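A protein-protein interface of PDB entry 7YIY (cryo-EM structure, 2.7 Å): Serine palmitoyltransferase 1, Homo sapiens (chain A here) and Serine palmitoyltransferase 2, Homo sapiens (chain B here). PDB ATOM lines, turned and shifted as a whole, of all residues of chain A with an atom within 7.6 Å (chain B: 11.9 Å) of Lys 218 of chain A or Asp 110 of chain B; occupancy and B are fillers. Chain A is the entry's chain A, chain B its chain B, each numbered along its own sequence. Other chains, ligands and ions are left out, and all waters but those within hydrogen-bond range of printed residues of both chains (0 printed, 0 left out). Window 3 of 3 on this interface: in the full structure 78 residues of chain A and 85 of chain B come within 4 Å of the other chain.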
ATOM      1  N   LEU A 171     -10.091 -36.530  18.764  1.00  0.00           N
ATOM      2  CA  LEU A 171     -10.332 -35.376  19.617  1.00  0.00           C
ATOM      3  C   LEU A 171      -9.119 -35.047  20.474  1.00  0.00           C
ATOM      4  O   LEU A 171      -8.843 -33.869  20.718  1.00  0.00           O
ATOM      5  CB  LEU A 171     -11.550 -35.625  20.506  1.00  0.00           C
ATOM      6  CG  LEU A 171     -12.955 -35.597  19.903  1.00  0.00           C
ATOM      7  CD1 LEU A 171     -13.951 -36.161  20.892  1.00  0.00           C
ATOM      8  CD2 LEU A 171     -13.357 -34.207  19.496  1.00  0.00           C
ATOM      9  N   GLU A 175      -6.285 -31.692  20.670  1.00  0.00           N
ATOM     10  CA  GLU A 175      -5.836 -30.981  21.858  1.00  0.00           C
ATOM     11  C   GLU A 175      -4.369 -30.578  21.753  1.00  0.00           C
ATOM     12  O   GLU A 175      -3.988 -29.500  22.191  1.00  0.00           O
ATOM     13  CB  GLU A 175      -6.053 -31.833  23.096  1.00  0.00           C
ATOM     14  CG  GLU A 175      -7.479 -31.809  23.591  1.00  0.00           C
ATOM     15  CD  GLU A 175      -7.607 -31.136  24.934  1.00  0.00           C
ATOM     16  OE1 GLU A 175      -8.423 -30.198  25.055  1.00  0.00           O
ATOM     17  OE2 GLU A 175      -6.891 -31.550  25.869  1.00  0.00           O
ATOM     18  N   THR A 188     -11.832 -21.216  16.623  1.00  0.00           N
ATOM     19  CA  THR A 188     -12.207 -22.374  15.822  1.00  0.00           C
ATOM     20  C   THR A 188     -13.327 -23.123  16.519  1.00  0.00           C
ATOM     21  O   THR A 188     -13.256 -23.375  17.724  1.00  0.00           O
ATOM     22  CB  THR A 188     -11.030 -23.322  15.573  1.00  0.00           C
ATOM     23  OG1 THR A 188     -10.659 -23.969  16.790  1.00  0.00           O
ATOM     24  CG2 THR A 188      -9.842 -22.564  15.029  1.00  0.00           C
ATOM     25  N   ARG A 189     -14.349 -23.483  15.755  1.00  0.00           N
ATOM     26  CA  ARG A 189     -15.501 -24.197  16.271  1.00  0.00           C
ATOM     27  C   ARG A 189     -15.449 -25.655  15.847  1.00  0.00           C
ATOM     28  O   ARG A 189     -14.912 -25.994  14.794  1.00  0.00           O
ATOM     29  CB  ARG A 189     -16.781 -23.533  15.777  1.00  0.00           C
ATOM     30  CG  ARG A 189     -16.852 -22.094  16.199  1.00  0.00           C
ATOM     31  CD  ARG A 189     -17.884 -21.302  15.459  1.00  0.00           C
ATOM     32  NE  ARG A 189     -17.866 -19.915  15.913  1.00  0.00           N
ATOM     33  CZ  ARG A 189     -17.066 -18.979  15.421  1.00  0.00           C
ATOM     34  NH1 ARG A 189     -17.109 -17.747  15.899  1.00  0.00           N
ATOM     35  NH2 ARG A 189     -16.225 -19.275  14.446  1.00  0.00           N
ATOM     36  N   ARG A 190     -15.999 -26.521  16.688  1.00  0.00           N
ATOM     37  CA  ARG A 190     -15.911 -27.959  16.495  1.00  0.00           C
ATOM     38  C   ARG A 190     -17.307 -28.549  16.435  1.00  0.00           C
ATOM     39  O   ARG A 190     -18.178 -28.168  17.216  1.00  0.00           O
ATOM     40  CB  ARG A 190     -15.130 -28.630  17.622  1.00  0.00           C
ATOM     41  CG  ARG A 190     -13.731 -28.127  17.799  1.00  0.00           C
ATOM     42  CD  ARG A 190     -13.692 -27.002  18.807  1.00  0.00           C
ATOM     43  NE  ARG A 190     -12.401 -26.328  18.817  1.00  0.00           N
ATOM     44  CZ  ARG A 190     -11.347 -26.756  19.495  1.00  0.00           C
ATOM     45  NH1 ARG A 190     -11.432 -27.860  20.221  1.00  0.00           N
ATOM     46  NH2 ARG A 190     -10.210 -26.085  19.442  1.00  0.00           N
ATOM     47  N   PHE A 191     -17.520 -29.471  15.505  1.00  0.00           N
ATOM     48  CA  PHE A 191     -18.803 -30.132  15.343  1.00  0.00           C
ATOM     49  C   PHE A 191     -18.595 -31.630  15.205  1.00  0.00           C
ATOM     50  O   PHE A 191     -17.600 -32.084  14.646  1.00  0.00           O
ATOM     51  CB  PHE A 191     -19.565 -29.604  14.117  1.00  0.00           C
ATOM     52  CG  PHE A 191     -19.665 -28.113  14.062  1.00  0.00           C
ATOM     53  CD1 PHE A 191     -20.698 -27.451  14.691  1.00  0.00           C
ATOM     54  CD2 PHE A 191     -18.721 -27.371  13.386  1.00  0.00           C
ATOM     55  CE1 PHE A 191     -20.783 -26.079  14.641  1.00  0.00           C
ATOM     56  CE2 PHE A 191     -18.806 -26.004  13.335  1.00  0.00           C
ATOM     57  CZ  PHE A 191     -19.836 -25.359  13.963  1.00  0.00           C
ATOM     58  N   ILE A 192     -19.545 -32.395  15.729  1.00  0.00           N
ATOM     59  CA  ILE A 192     -19.600 -33.841  15.548  1.00  0.00           C
ATOM     60  C   ILE A 192     -20.895 -34.119  14.799  1.00  0.00           C
ATOM     61  O   ILE A 192     -21.976 -33.757  15.266  1.00  0.00           O
ATOM     62  CB  ILE A 192     -19.557 -34.604  16.875  1.00  0.00           C
ATOM     63  CG1 ILE A 192     -18.267 -34.300  17.628  1.00  0.00           C
ATOM     64  CG2 ILE A 192     -19.668 -36.087  16.631  1.00  0.00           C
ATOM     65  CD1 ILE A 192     -18.279 -34.786  19.048  1.00  0.00           C
ATOM     66  N   LYS A 212     -21.268 -37.501  26.557  1.00  0.00           N
ATOM     67  CA  LYS A 212     -20.182 -37.320  27.514  1.00  0.00           C
ATOM     68  C   LYS A 212     -18.905 -36.793  26.880  1.00  0.00           C
ATOM     69  O   LYS A 212     -18.180 -36.036  27.528  1.00  0.00           O
ATOM     70  CB  LYS A 212     -19.883 -38.635  28.223  1.00  0.00           C
ATOM     71  CG  LYS A 212     -20.989 -39.098  29.124  1.00  0.00           C
ATOM     72  CD  LYS A 212     -20.473 -40.026  30.193  1.00  0.00           C
ATOM     73  CE  LYS A 212     -21.608 -40.841  30.785  1.00  0.00           C
ATOM     74  NZ  LYS A 212     -21.792 -42.137  30.078  1.00  0.00           N
ATOM     75  N   LEU A 213     -18.595 -37.194  25.655  1.00  0.00           N
ATOM     76  CA  LEU A 213     -17.475 -36.633  24.916  1.00  0.00           C
ATOM     77  C   LEU A 213     -17.697 -35.176  24.550  1.00  0.00           C
ATOM     78  O   LEU A 213     -16.736 -34.394  24.549  1.00  0.00           O
ATOM     79  CB  LEU A 213     -17.231 -37.449  23.643  1.00  0.00           C
ATOM     80  CG  LEU A 213     -16.463 -38.761  23.809  1.00  0.00           C
ATOM     81  CD1 LEU A 213     -16.183 -39.377  22.470  1.00  0.00           C
ATOM     82  CD2 LEU A 213     -15.180 -38.540  24.562  1.00  0.00           C
ATOM     83  N   LYS A 214     -18.942 -34.807  24.238  1.00  0.00           N
ATOM     84  CA  LYS A 214     -19.290 -33.424  23.925  1.00  0.00           C
ATOM     85  C   LYS A 214     -18.891 -32.446  25.015  1.00  0.00           C
ATOM     86  O   LYS A 214     -18.329 -31.391  24.714  1.00  0.00           O
ATOM     87  CB  LYS A 214     -20.789 -33.299  23.690  1.00  0.00           C
ATOM     88  CG  LYS A 214     -21.292 -31.885  23.815  1.00  0.00           C
ATOM     89  CD  LYS A 214     -22.761 -31.787  23.526  1.00  0.00           C
ATOM     90  CE  LYS A 214     -23.220 -30.359  23.602  1.00  0.00           C
ATOM     91  NZ  LYS A 214     -24.628 -30.232  23.171  1.00  0.00           N
ATOM     92  N   TYR A 215     -19.184 -32.759  26.269  1.00  0.00           N
ATOM     93  CA  TYR A 215     -18.907 -31.839  27.358  1.00  0.00           C
ATOM     94  C   TYR A 215     -17.466 -31.891  27.826  1.00  0.00           C
ATOM     95  O   TYR A 215     -17.040 -31.009  28.577  1.00  0.00           O
ATOM     96  CB  TYR A 215     -19.845 -32.125  28.525  1.00  0.00           C
ATOM     97  CG  TYR A 215     -21.238 -31.623  28.270  1.00  0.00           C
ATOM     98  CD1 TYR A 215     -21.492 -30.268  28.140  1.00  0.00           C
ATOM     99  CD2 TYR A 215     -22.294 -32.503  28.126  1.00  0.00           C
ATOM    100  CE1 TYR A 215     -22.761 -29.804  27.896  1.00  0.00           C
ATOM    101  CE2 TYR A 215     -23.568 -32.049  27.880  1.00  0.00           C
ATOM    102  CZ  TYR A 215     -23.797 -30.699  27.762  1.00  0.00           C
ATOM    103  OH  TYR A 215     -25.069 -30.246  27.517  1.00  0.00           O
ATOM    104  N   LYS A 216     -16.707 -32.885  27.391  1.00  0.00           N
ATOM    105  CA  LYS A 216     -15.304 -32.991  27.750  1.00  0.00           C
ATOM    106  C   LYS A 216     -14.410 -32.280  26.751  1.00  0.00           C
ATOM    107  O   LYS A 216     -13.415 -31.665  27.141  1.00  0.00           O
ATOM    108  CB  LYS A 216     -14.912 -34.461  27.862  1.00  0.00           C
ATOM    109  CG  LYS A 216     -13.513 -34.694  28.352  1.00  0.00           C
ATOM    110  CD  LYS A 216     -13.250 -36.172  28.492  1.00  0.00           C
ATOM    111  CE  LYS A 216     -11.810 -36.442  28.860  1.00  0.00           C
ATOM    112  NZ  LYS A 216     -11.531 -37.899  28.916  1.00  0.00           N
ATOM    113  N   TYR A 217     -14.749 -32.332  25.463  1.00  0.00           N
ATOM    114  CA  TYR A 217     -13.913 -31.708  24.448  1.00  0.00           C
ATOM    115  C   TYR A 217     -14.578 -30.510  23.783  1.00  0.00           C
ATOM    116  O   TYR A 217     -14.022 -29.951  22.835  1.00  0.00           O
ATOM    117  CB  TYR A 217     -13.492 -32.743  23.409  1.00  0.00           C
ATOM    118  CG  TYR A 217     -12.671 -33.856  24.007  1.00  0.00           C
ATOM    119  CD1 TYR A 217     -11.307 -33.720  24.169  1.00  0.00           C
ATOM    120  CD2 TYR A 217     -13.261 -35.033  24.419  1.00  0.00           C
ATOM    121  CE1 TYR A 217     -10.559 -34.718  24.722  1.00  0.00           C
ATOM    122  CE2 TYR A 217     -12.516 -36.043  24.969  1.00  0.00           C
ATOM    123  CZ  TYR A 217     -11.167 -35.878  25.120  1.00  0.00           C
ATOM    124  OH  TYR A 217     -10.418 -36.883  25.674  1.00  0.00           O
ATOM    125  N   LYS A 218     -15.746 -30.103  24.266  1.00  0.00           N
ATOM    126  CA  LYS A 218     -16.418 -28.871  23.853  1.00  0.00           C
ATOM    127  C   LYS A 218     -16.710 -28.848  22.354  1.00  0.00           C
ATOM    128  O   LYS A 218     -16.320 -27.934  21.631  1.00  0.00           O
ATOM    129  CB  LYS A 218     -15.600 -27.647  24.256  1.00  0.00           C
ATOM    130  CG  LYS A 218     -15.814 -27.173  25.673  1.00  0.00           C
ATOM    131  CD  LYS A 218     -15.080 -28.039  26.658  1.00  0.00           C
ATOM    132  CE  LYS A 218     -15.225 -27.513  28.068  1.00  0.00           C
ATOM    133  NZ  LYS A 218     -14.627 -28.443  29.064  1.00  0.00           N
ATOM    134  N   ALA A 219     -17.429 -29.865  21.893  1.00  0.00           N
ATOM    135  CA  ALA A 219     -17.866 -29.943  20.508  1.00  0.00           C
ATOM    136  C   ALA A 219     -19.374 -30.138  20.448  1.00  0.00           C
ATOM    137  O   ALA A 219     -19.950 -30.873  21.247  1.00  0.00           O
ATOM    138  CB  ALA A 219     -17.160 -31.077  19.770  1.00  0.00           C
ATOM    139  N   ARG A 220     -20.010 -29.468  19.496  1.00  0.00           N
ATOM    140  CA  ARG A 220     -21.456 -29.507  19.327  1.00  0.00           C
ATOM    141  C   ARG A 220     -21.846 -30.657  18.410  1.00  0.00           C
ATOM    142  O   ARG A 220     -21.095 -31.016  17.504  1.00  0.00           O
ATOM    143  CB  ARG A 220     -21.962 -28.183  18.759  1.00  0.00           C
ATOM    144  CG  ARG A 220     -21.808 -27.020  19.708  1.00  0.00           C
ATOM    145  CD  ARG A 220     -22.201 -25.716  19.066  1.00  0.00           C
ATOM    146  NE  ARG A 220     -22.196 -24.616  20.023  1.00  0.00           N
ATOM    147  CZ  ARG A 220     -21.172 -23.796  20.224  1.00  0.00           C
ATOM    148  NH1 ARG A 220     -21.263 -22.830  21.117  1.00  0.00           N
ATOM    149  NH2 ARG A 220     -20.061 -23.930  19.521  1.00  0.00           N
ATOM    150  N   THR B 103     -30.116 -16.333  23.584  1.00  0.00           N
ATOM    151  CA  THR B 103     -28.781 -16.478  24.142  1.00  0.00           C
ATOM    152  C   THR B 103     -28.437 -17.954  24.260  1.00  0.00           C
ATOM    153  O   THR B 103     -29.307 -18.824  24.249  1.00  0.00           O
ATOM    154  CB  THR B 103     -28.663 -15.799  25.514  1.00  0.00           C
ATOM    155  OG1 THR B 103     -29.797 -16.136  26.315  1.00  0.00           O
ATOM    156  CG2 THR B 103     -28.593 -14.292  25.361  1.00  0.00           C
ATOM    157  N   GLU B 104     -27.144 -18.224  24.386  1.00  0.00           N
ATOM    158  CA  GLU B 104     -26.646 -19.577  24.560  1.00  0.00           C
ATOM    159  C   GLU B 104     -27.118 -20.156  25.897  1.00  0.00           C
ATOM    160  O   GLU B 104     -27.445 -19.431  26.838  1.00  0.00           O
ATOM    161  CB  GLU B 104     -25.119 -19.578  24.479  1.00  0.00           C
ATOM    162  CG  GLU B 104     -24.465 -20.929  24.607  1.00  0.00           C
ATOM    163  CD  GLU B 104     -24.788 -21.850  23.462  1.00  0.00           C
ATOM    164  OE1 GLU B 104     -24.924 -21.368  22.326  1.00  0.00           O
ATOM    165  OE2 GLU B 104     -24.924 -23.063  23.701  1.00  0.00           O
ATOM    166  N   ARG B 105     -27.174 -21.483  25.964  1.00  0.00           N
ATOM    167  CA  ARG B 105     -27.452 -22.179  27.207  1.00  0.00           C
ATOM    168  C   ARG B 105     -26.410 -21.829  28.263  1.00  0.00           C
ATOM    169  O   ARG B 105     -25.294 -21.406  27.962  1.00  0.00           O
ATOM    170  CB  ARG B 105     -27.454 -23.693  27.006  1.00  0.00           C
ATOM    171  CG  ARG B 105     -28.526 -24.222  26.102  1.00  0.00           C
ATOM    172  CD  ARG B 105     -28.378 -25.717  25.854  1.00  0.00           C
ATOM    173  NE  ARG B 105     -28.752 -26.519  27.011  1.00  0.00           N
ATOM    174  CZ  ARG B 105     -27.991 -27.464  27.552  1.00  0.00           C
ATOM    175  NH1 ARG B 105     -26.806 -27.742  27.040  1.00  0.00           N
ATOM    176  NH2 ARG B 105     -28.424 -28.137  28.604  1.00  0.00           N
ATOM    177  N   GLU B 106     -26.800 -22.013  29.524  1.00  0.00           N
ATOM    178  CA  GLU B 106     -25.866 -21.834  30.627  1.00  0.00           C
ATOM    179  C   GLU B 106     -24.780 -22.901  30.628  1.00  0.00           C
ATOM    180  O   GLU B 106     -23.624 -22.604  30.939  1.00  0.00           O
ATOM    181  CB  GLU B 106     -26.628 -21.843  31.950  1.00  0.00           C
ATOM    182  CG  GLU B 106     -25.760 -21.708  33.182  1.00  0.00           C
ATOM    183  CD  GLU B 106     -25.522 -20.269  33.575  1.00  0.00           C
ATOM    184  OE1 GLU B 106     -26.306 -19.399  33.143  1.00  0.00           O
ATOM    185  OE2 GLU B 106     -24.556 -20.007  34.323  1.00  0.00           O
ATOM    186  N   GLU B 107     -25.124 -24.140  30.277  1.00  0.00           N
ATOM    187  CA  GLU B 107     -24.161 -25.233  30.340  1.00  0.00           C
ATOM    188  C   GLU B 107     -23.103 -25.158  29.249  1.00  0.00           C
ATOM    189  O   GLU B 107     -22.131 -25.914  29.301  1.00  0.00           O
ATOM    190  CB  GLU B 107     -24.888 -26.573  30.262  1.00  0.00           C
ATOM    191  CG  GLU B 107     -25.773 -26.857  31.454  1.00  0.00           C
ATOM    192  CD  GLU B 107     -27.166 -26.290  31.303  1.00  0.00           C
ATOM    193  OE1 GLU B 107     -28.137 -27.058  31.436  1.00  0.00           O
ATOM    194  OE2 GLU B 107     -27.294 -25.078  31.045  1.00  0.00           O
ATOM    195  N   GLN B 108     -23.266 -24.279  28.267  1.00  0.00           N
ATOM    196  CA  GLN B 108     -22.329 -24.147  27.160  1.00  0.00           C
ATOM    197  C   GLN B 108     -21.762 -22.735  27.069  1.00  0.00           C
ATOM    198  O   GLN B 108     -21.635 -22.167  25.985  1.00  0.00           O
ATOM    199  CB  GLN B 108     -22.992 -24.544  25.849  1.00  0.00           C
ATOM    200  CG  GLN B 108     -23.485 -25.974  25.835  1.00  0.00           C
ATOM    201  CD  GLN B 108     -24.071 -26.375  24.504  1.00  0.00           C
ATOM    202  OE1 GLN B 108     -25.016 -27.152  24.440  1.00  0.00           O
ATOM    203  NE2 GLN B 108     -23.517 -25.838  23.432  1.00  0.00           N
ATOM    204  N   LYS B 109     -21.377 -22.185  28.214  1.00  0.00           N
ATOM    205  CA  LYS B 109     -20.809 -20.846  28.273  1.00  0.00           C
ATOM    206  C   LYS B 109     -19.307 -20.860  28.019  1.00  0.00           C
ATOM    207  O   LYS B 109     -18.732 -19.854  27.620  1.00  0.00           O
ATOM    208  CB  LYS B 109     -21.086 -20.209  29.631  1.00  0.00           C
ATOM    209  CG  LYS B 109     -22.484 -19.644  29.786  1.00  0.00           C
ATOM    210  CD  LYS B 109     -22.939 -19.736  31.231  1.00  0.00           C
ATOM    211  CE  LYS B 109     -21.811 -19.383  32.188  1.00  0.00           C
ATOM    212  NZ  LYS B 109     -20.919 -20.543  32.474  1.00  0.00           N
ATOM    213  N   ASP B 110     -18.675 -22.003  28.259  1.00  0.00           N
ATOM    214  CA  ASP B 110     -17.242 -22.158  28.061  1.00  0.00           C
ATOM    215  C   ASP B 110     -16.893 -22.773  26.712  1.00  0.00           C
ATOM    216  O   ASP B 110     -15.730 -23.113  26.482  1.00  0.00           O
ATOM    217  CB  ASP B 110     -16.648 -22.992  29.195  1.00  0.00           C
ATOM    218  CG  ASP B 110     -17.461 -24.233  29.495  1.00  0.00           C
ATOM    219  OD1 ASP B 110     -16.860 -25.306  29.698  1.00  0.00           O
ATOM    220  OD2 ASP B 110     -18.704 -24.135  29.539  1.00  0.00           O
ATOM    221  N   PHE B 111     -17.868 -22.927  25.826  1.00  0.00           N
ATOM    222  CA  PHE B 111     -17.627 -23.302  24.444  1.00  0.00           C
ATOM    223  C   PHE B 111     -17.120 -22.088  23.672  1.00  0.00           C
ATOM    224  O   PHE B 111     -17.171 -20.956  24.150  1.00  0.00           O
ATOM    225  CB  PHE B 111     -18.912 -23.820  23.796  1.00  0.00           C
ATOM    226  CG  PHE B 111     -19.294 -25.219  24.189  1.00  0.00           C
ATOM    227  CD1 PHE B 111     -19.188 -25.653  25.493  1.00  0.00           C
ATOM    228  CD2 PHE B 111     -19.793 -26.093  23.248  1.00  0.00           C
ATOM    229  CE1 PHE B 111     -19.554 -26.928  25.842  1.00  0.00           C
ATOM    230  CE2 PHE B 111     -20.158 -27.370  23.599  1.00  0.00           C
ATOM    231  CZ  PHE B 111     -20.037 -27.784  24.896  1.00  0.00           C
ATOM    232  N   VAL B 112     -16.636 -22.322  22.466  1.00  0.00           N
ATOM    233  CA  VAL B 112     -16.415 -21.231  21.525  1.00  0.00           C
ATOM    234  C   VAL B 112     -17.771 -20.753  21.031  1.00  0.00           C
ATOM    235  O   VAL B 112     -18.655 -21.565  20.741  1.00  0.00           O
ATOM    236  CB  VAL B 112     -15.519 -21.688  20.359  1.00  0.00           C
ATOM    237  CG1 VAL B 112     -15.413 -20.610  19.312  1.00  0.00           C
ATOM    238  CG2 VAL B 112     -14.152 -22.082  20.860  1.00  0.00           C
ATOM    239  N   SER B 113     -17.951 -19.438  20.938  1.00  0.00           N
ATOM    240  CA  SER B 113     -19.255 -18.894  20.588  1.00  0.00           C
ATOM    241  C   SER B 113     -19.670 -19.349  19.196  1.00  0.00           C
ATOM    242  O   SER B 113     -18.839 -19.502  18.301  1.00  0.00           O
ATOM    243  CB  SER B 113     -19.235 -17.369  20.659  1.00  0.00           C
ATOM    244  OG  SER B 113     -18.496 -16.818  19.591  1.00  0.00           O
ATOM    245  N   LEU B 114     -20.975 -19.562  19.023  1.00  0.00           N
ATOM    246  CA  LEU B 114     -21.477 -20.154  17.791  1.00  0.00           C
ATOM    247  C   LEU B 114     -21.379 -19.205  16.606  1.00  0.00           C
ATOM    248  O   LEU B 114     -21.118 -19.650  15.486  1.00  0.00           O
ATOM    249  CB  LEU B 114     -22.921 -20.612  17.990  1.00  0.00           C
ATOM    250  CG  LEU B 114     -23.532 -21.507  16.917  1.00  0.00           C
ATOM    251  CD1 LEU B 114     -22.738 -22.772  16.744  1.00  0.00           C
ATOM    252  CD2 LEU B 114     -24.949 -21.823  17.283  1.00  0.00           C
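NH1 of Arg 105 of chain B lies within hydrogen-bond range of OH of Tyr 215 of chain A (3.1 Å). The side-chain amino group (NZ) of Lys 214 of chain A sits at hydrogen-bond distance from the side-chain amide oxygen (OE1) of Gln 108 of chain B. OD1 of Asp 110 of chain B is in salt-bridge range of NZ of Lys 218 of chain A, 3.9 Å away. NH1 of Arg 220 of chain A is in hydrogen-bond range of O of Val 112 of chain B (2.9 Å). The backbone carbonyl oxygen (O) of Ser 113 of chain B sits at hydrogen-bond distance from the guanidinium group (NE) of Arg 189 of chain A. O of Leu 114 of chain B is in hydrogen-bond range of NE of Arg 189 of chain A, at 3.3 Å.
The side-chain amide nitrogen (NE2) of Gln 108 of chain B sits at hydrogen-bond distance from the side-chain carboxylate (OE2) of Glu 104 of chain B, at 3.1 Å. OE1 of Gln 108 of chain B sits at hydrogen-bond distance from NH1 of Arg 105 of chain B (3.2 Å). The backbone carbonyl oxygen of Thr 188 of chain A sits at hydrogen-bond distance from the guanidinium group of Arg 190 of chain A, 3.3 Å away. The backbone NH of Arg 220 of chain A sits at hydrogen-bond distance from the backbone carbonyl oxygen of Arg 190 of chain A (3.2 Å). The backbone carbonyl oxygen (O) of Arg 220 of chain A sits at hydrogen-bond distance from the backbone NH (N) of Ile 192 of chain A, 2.7 Å away. N of Ala 219 of chain A sits at hydrogen-bond distance from O of Lys 214 of chain A (3.3 Å).
Thr 188 of chain A touches Val 112 of chain B. Arg 189 of chain A touches Val 112 of chain B (CG to CG1, 3.7 Å). Lys 214 of chain A touches Phe 111 of chain B. Lys 218 of chain A touches Phe 111 of chain B. Gln 108 of chain B touches Arg 220 of chain A (NE2 to NE, 3.9 Å). Phe 111 of chain B touches Arg 220 of chain A. Leu 114 of chain B touches Arg 220 of chain A (CD1 to CD, 3.8 Å).
Lys 218 of chain A touches two residues of chain B. Printed residues of chain A within 4 Å of Asp 110 of chain B: Lys 218 (3.2 Å). No residue of chain B comes within 4 Å of Arg 190 of chain A. No residue of chain B comes within 4 Å of Ala 219 of chain A. Arg 220 of chain A touches just these residues of chain B: Gln 108, Phe 111, Val 112 and Leu 114. Of the printed residues of chain B, Lys 214 of chain A touches Gln 108 (3.4 Å) and Phe 111 (3.995 Å). Of the printed residues of chain A, Phe 111 of chain B touches Lys 214 (3.995 Å), Lys 218 (3.7 Å) and Arg 220 (3.7 Å). Of the printed residues of chain B, Arg 189 of chain A touches Val 112 (3.7 Å), Ser 113 (2.6 Å) and Leu 114 (3.3 Å). Printed residues of chain A within 4 Å of Val 112 of chain B: Thr 188 (3.5 Å), Arg 189 (3.7 Å) and Arg 220 (2.9 Å). Printed residues of chain A within 4 Å of Arg 105 of chain B: Tyr 215 (3.1 Å). The nearest residue of chain B that does not touch Lys 218 of chain A is Val 112 of chain B (5.7 Å).
Hydrophobic or aromatic side chains of chain A that line the printed part of chain B: Tyr 215. Along chain A the printed residues that touch a printed residue of chain B span positions 188 to 220. Printed residues of chain B that touch a printed residue of chain A: Arg 105, Gln 108, Asp 110, Phe 111, Val 112, Ser 113 and Leu 114.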
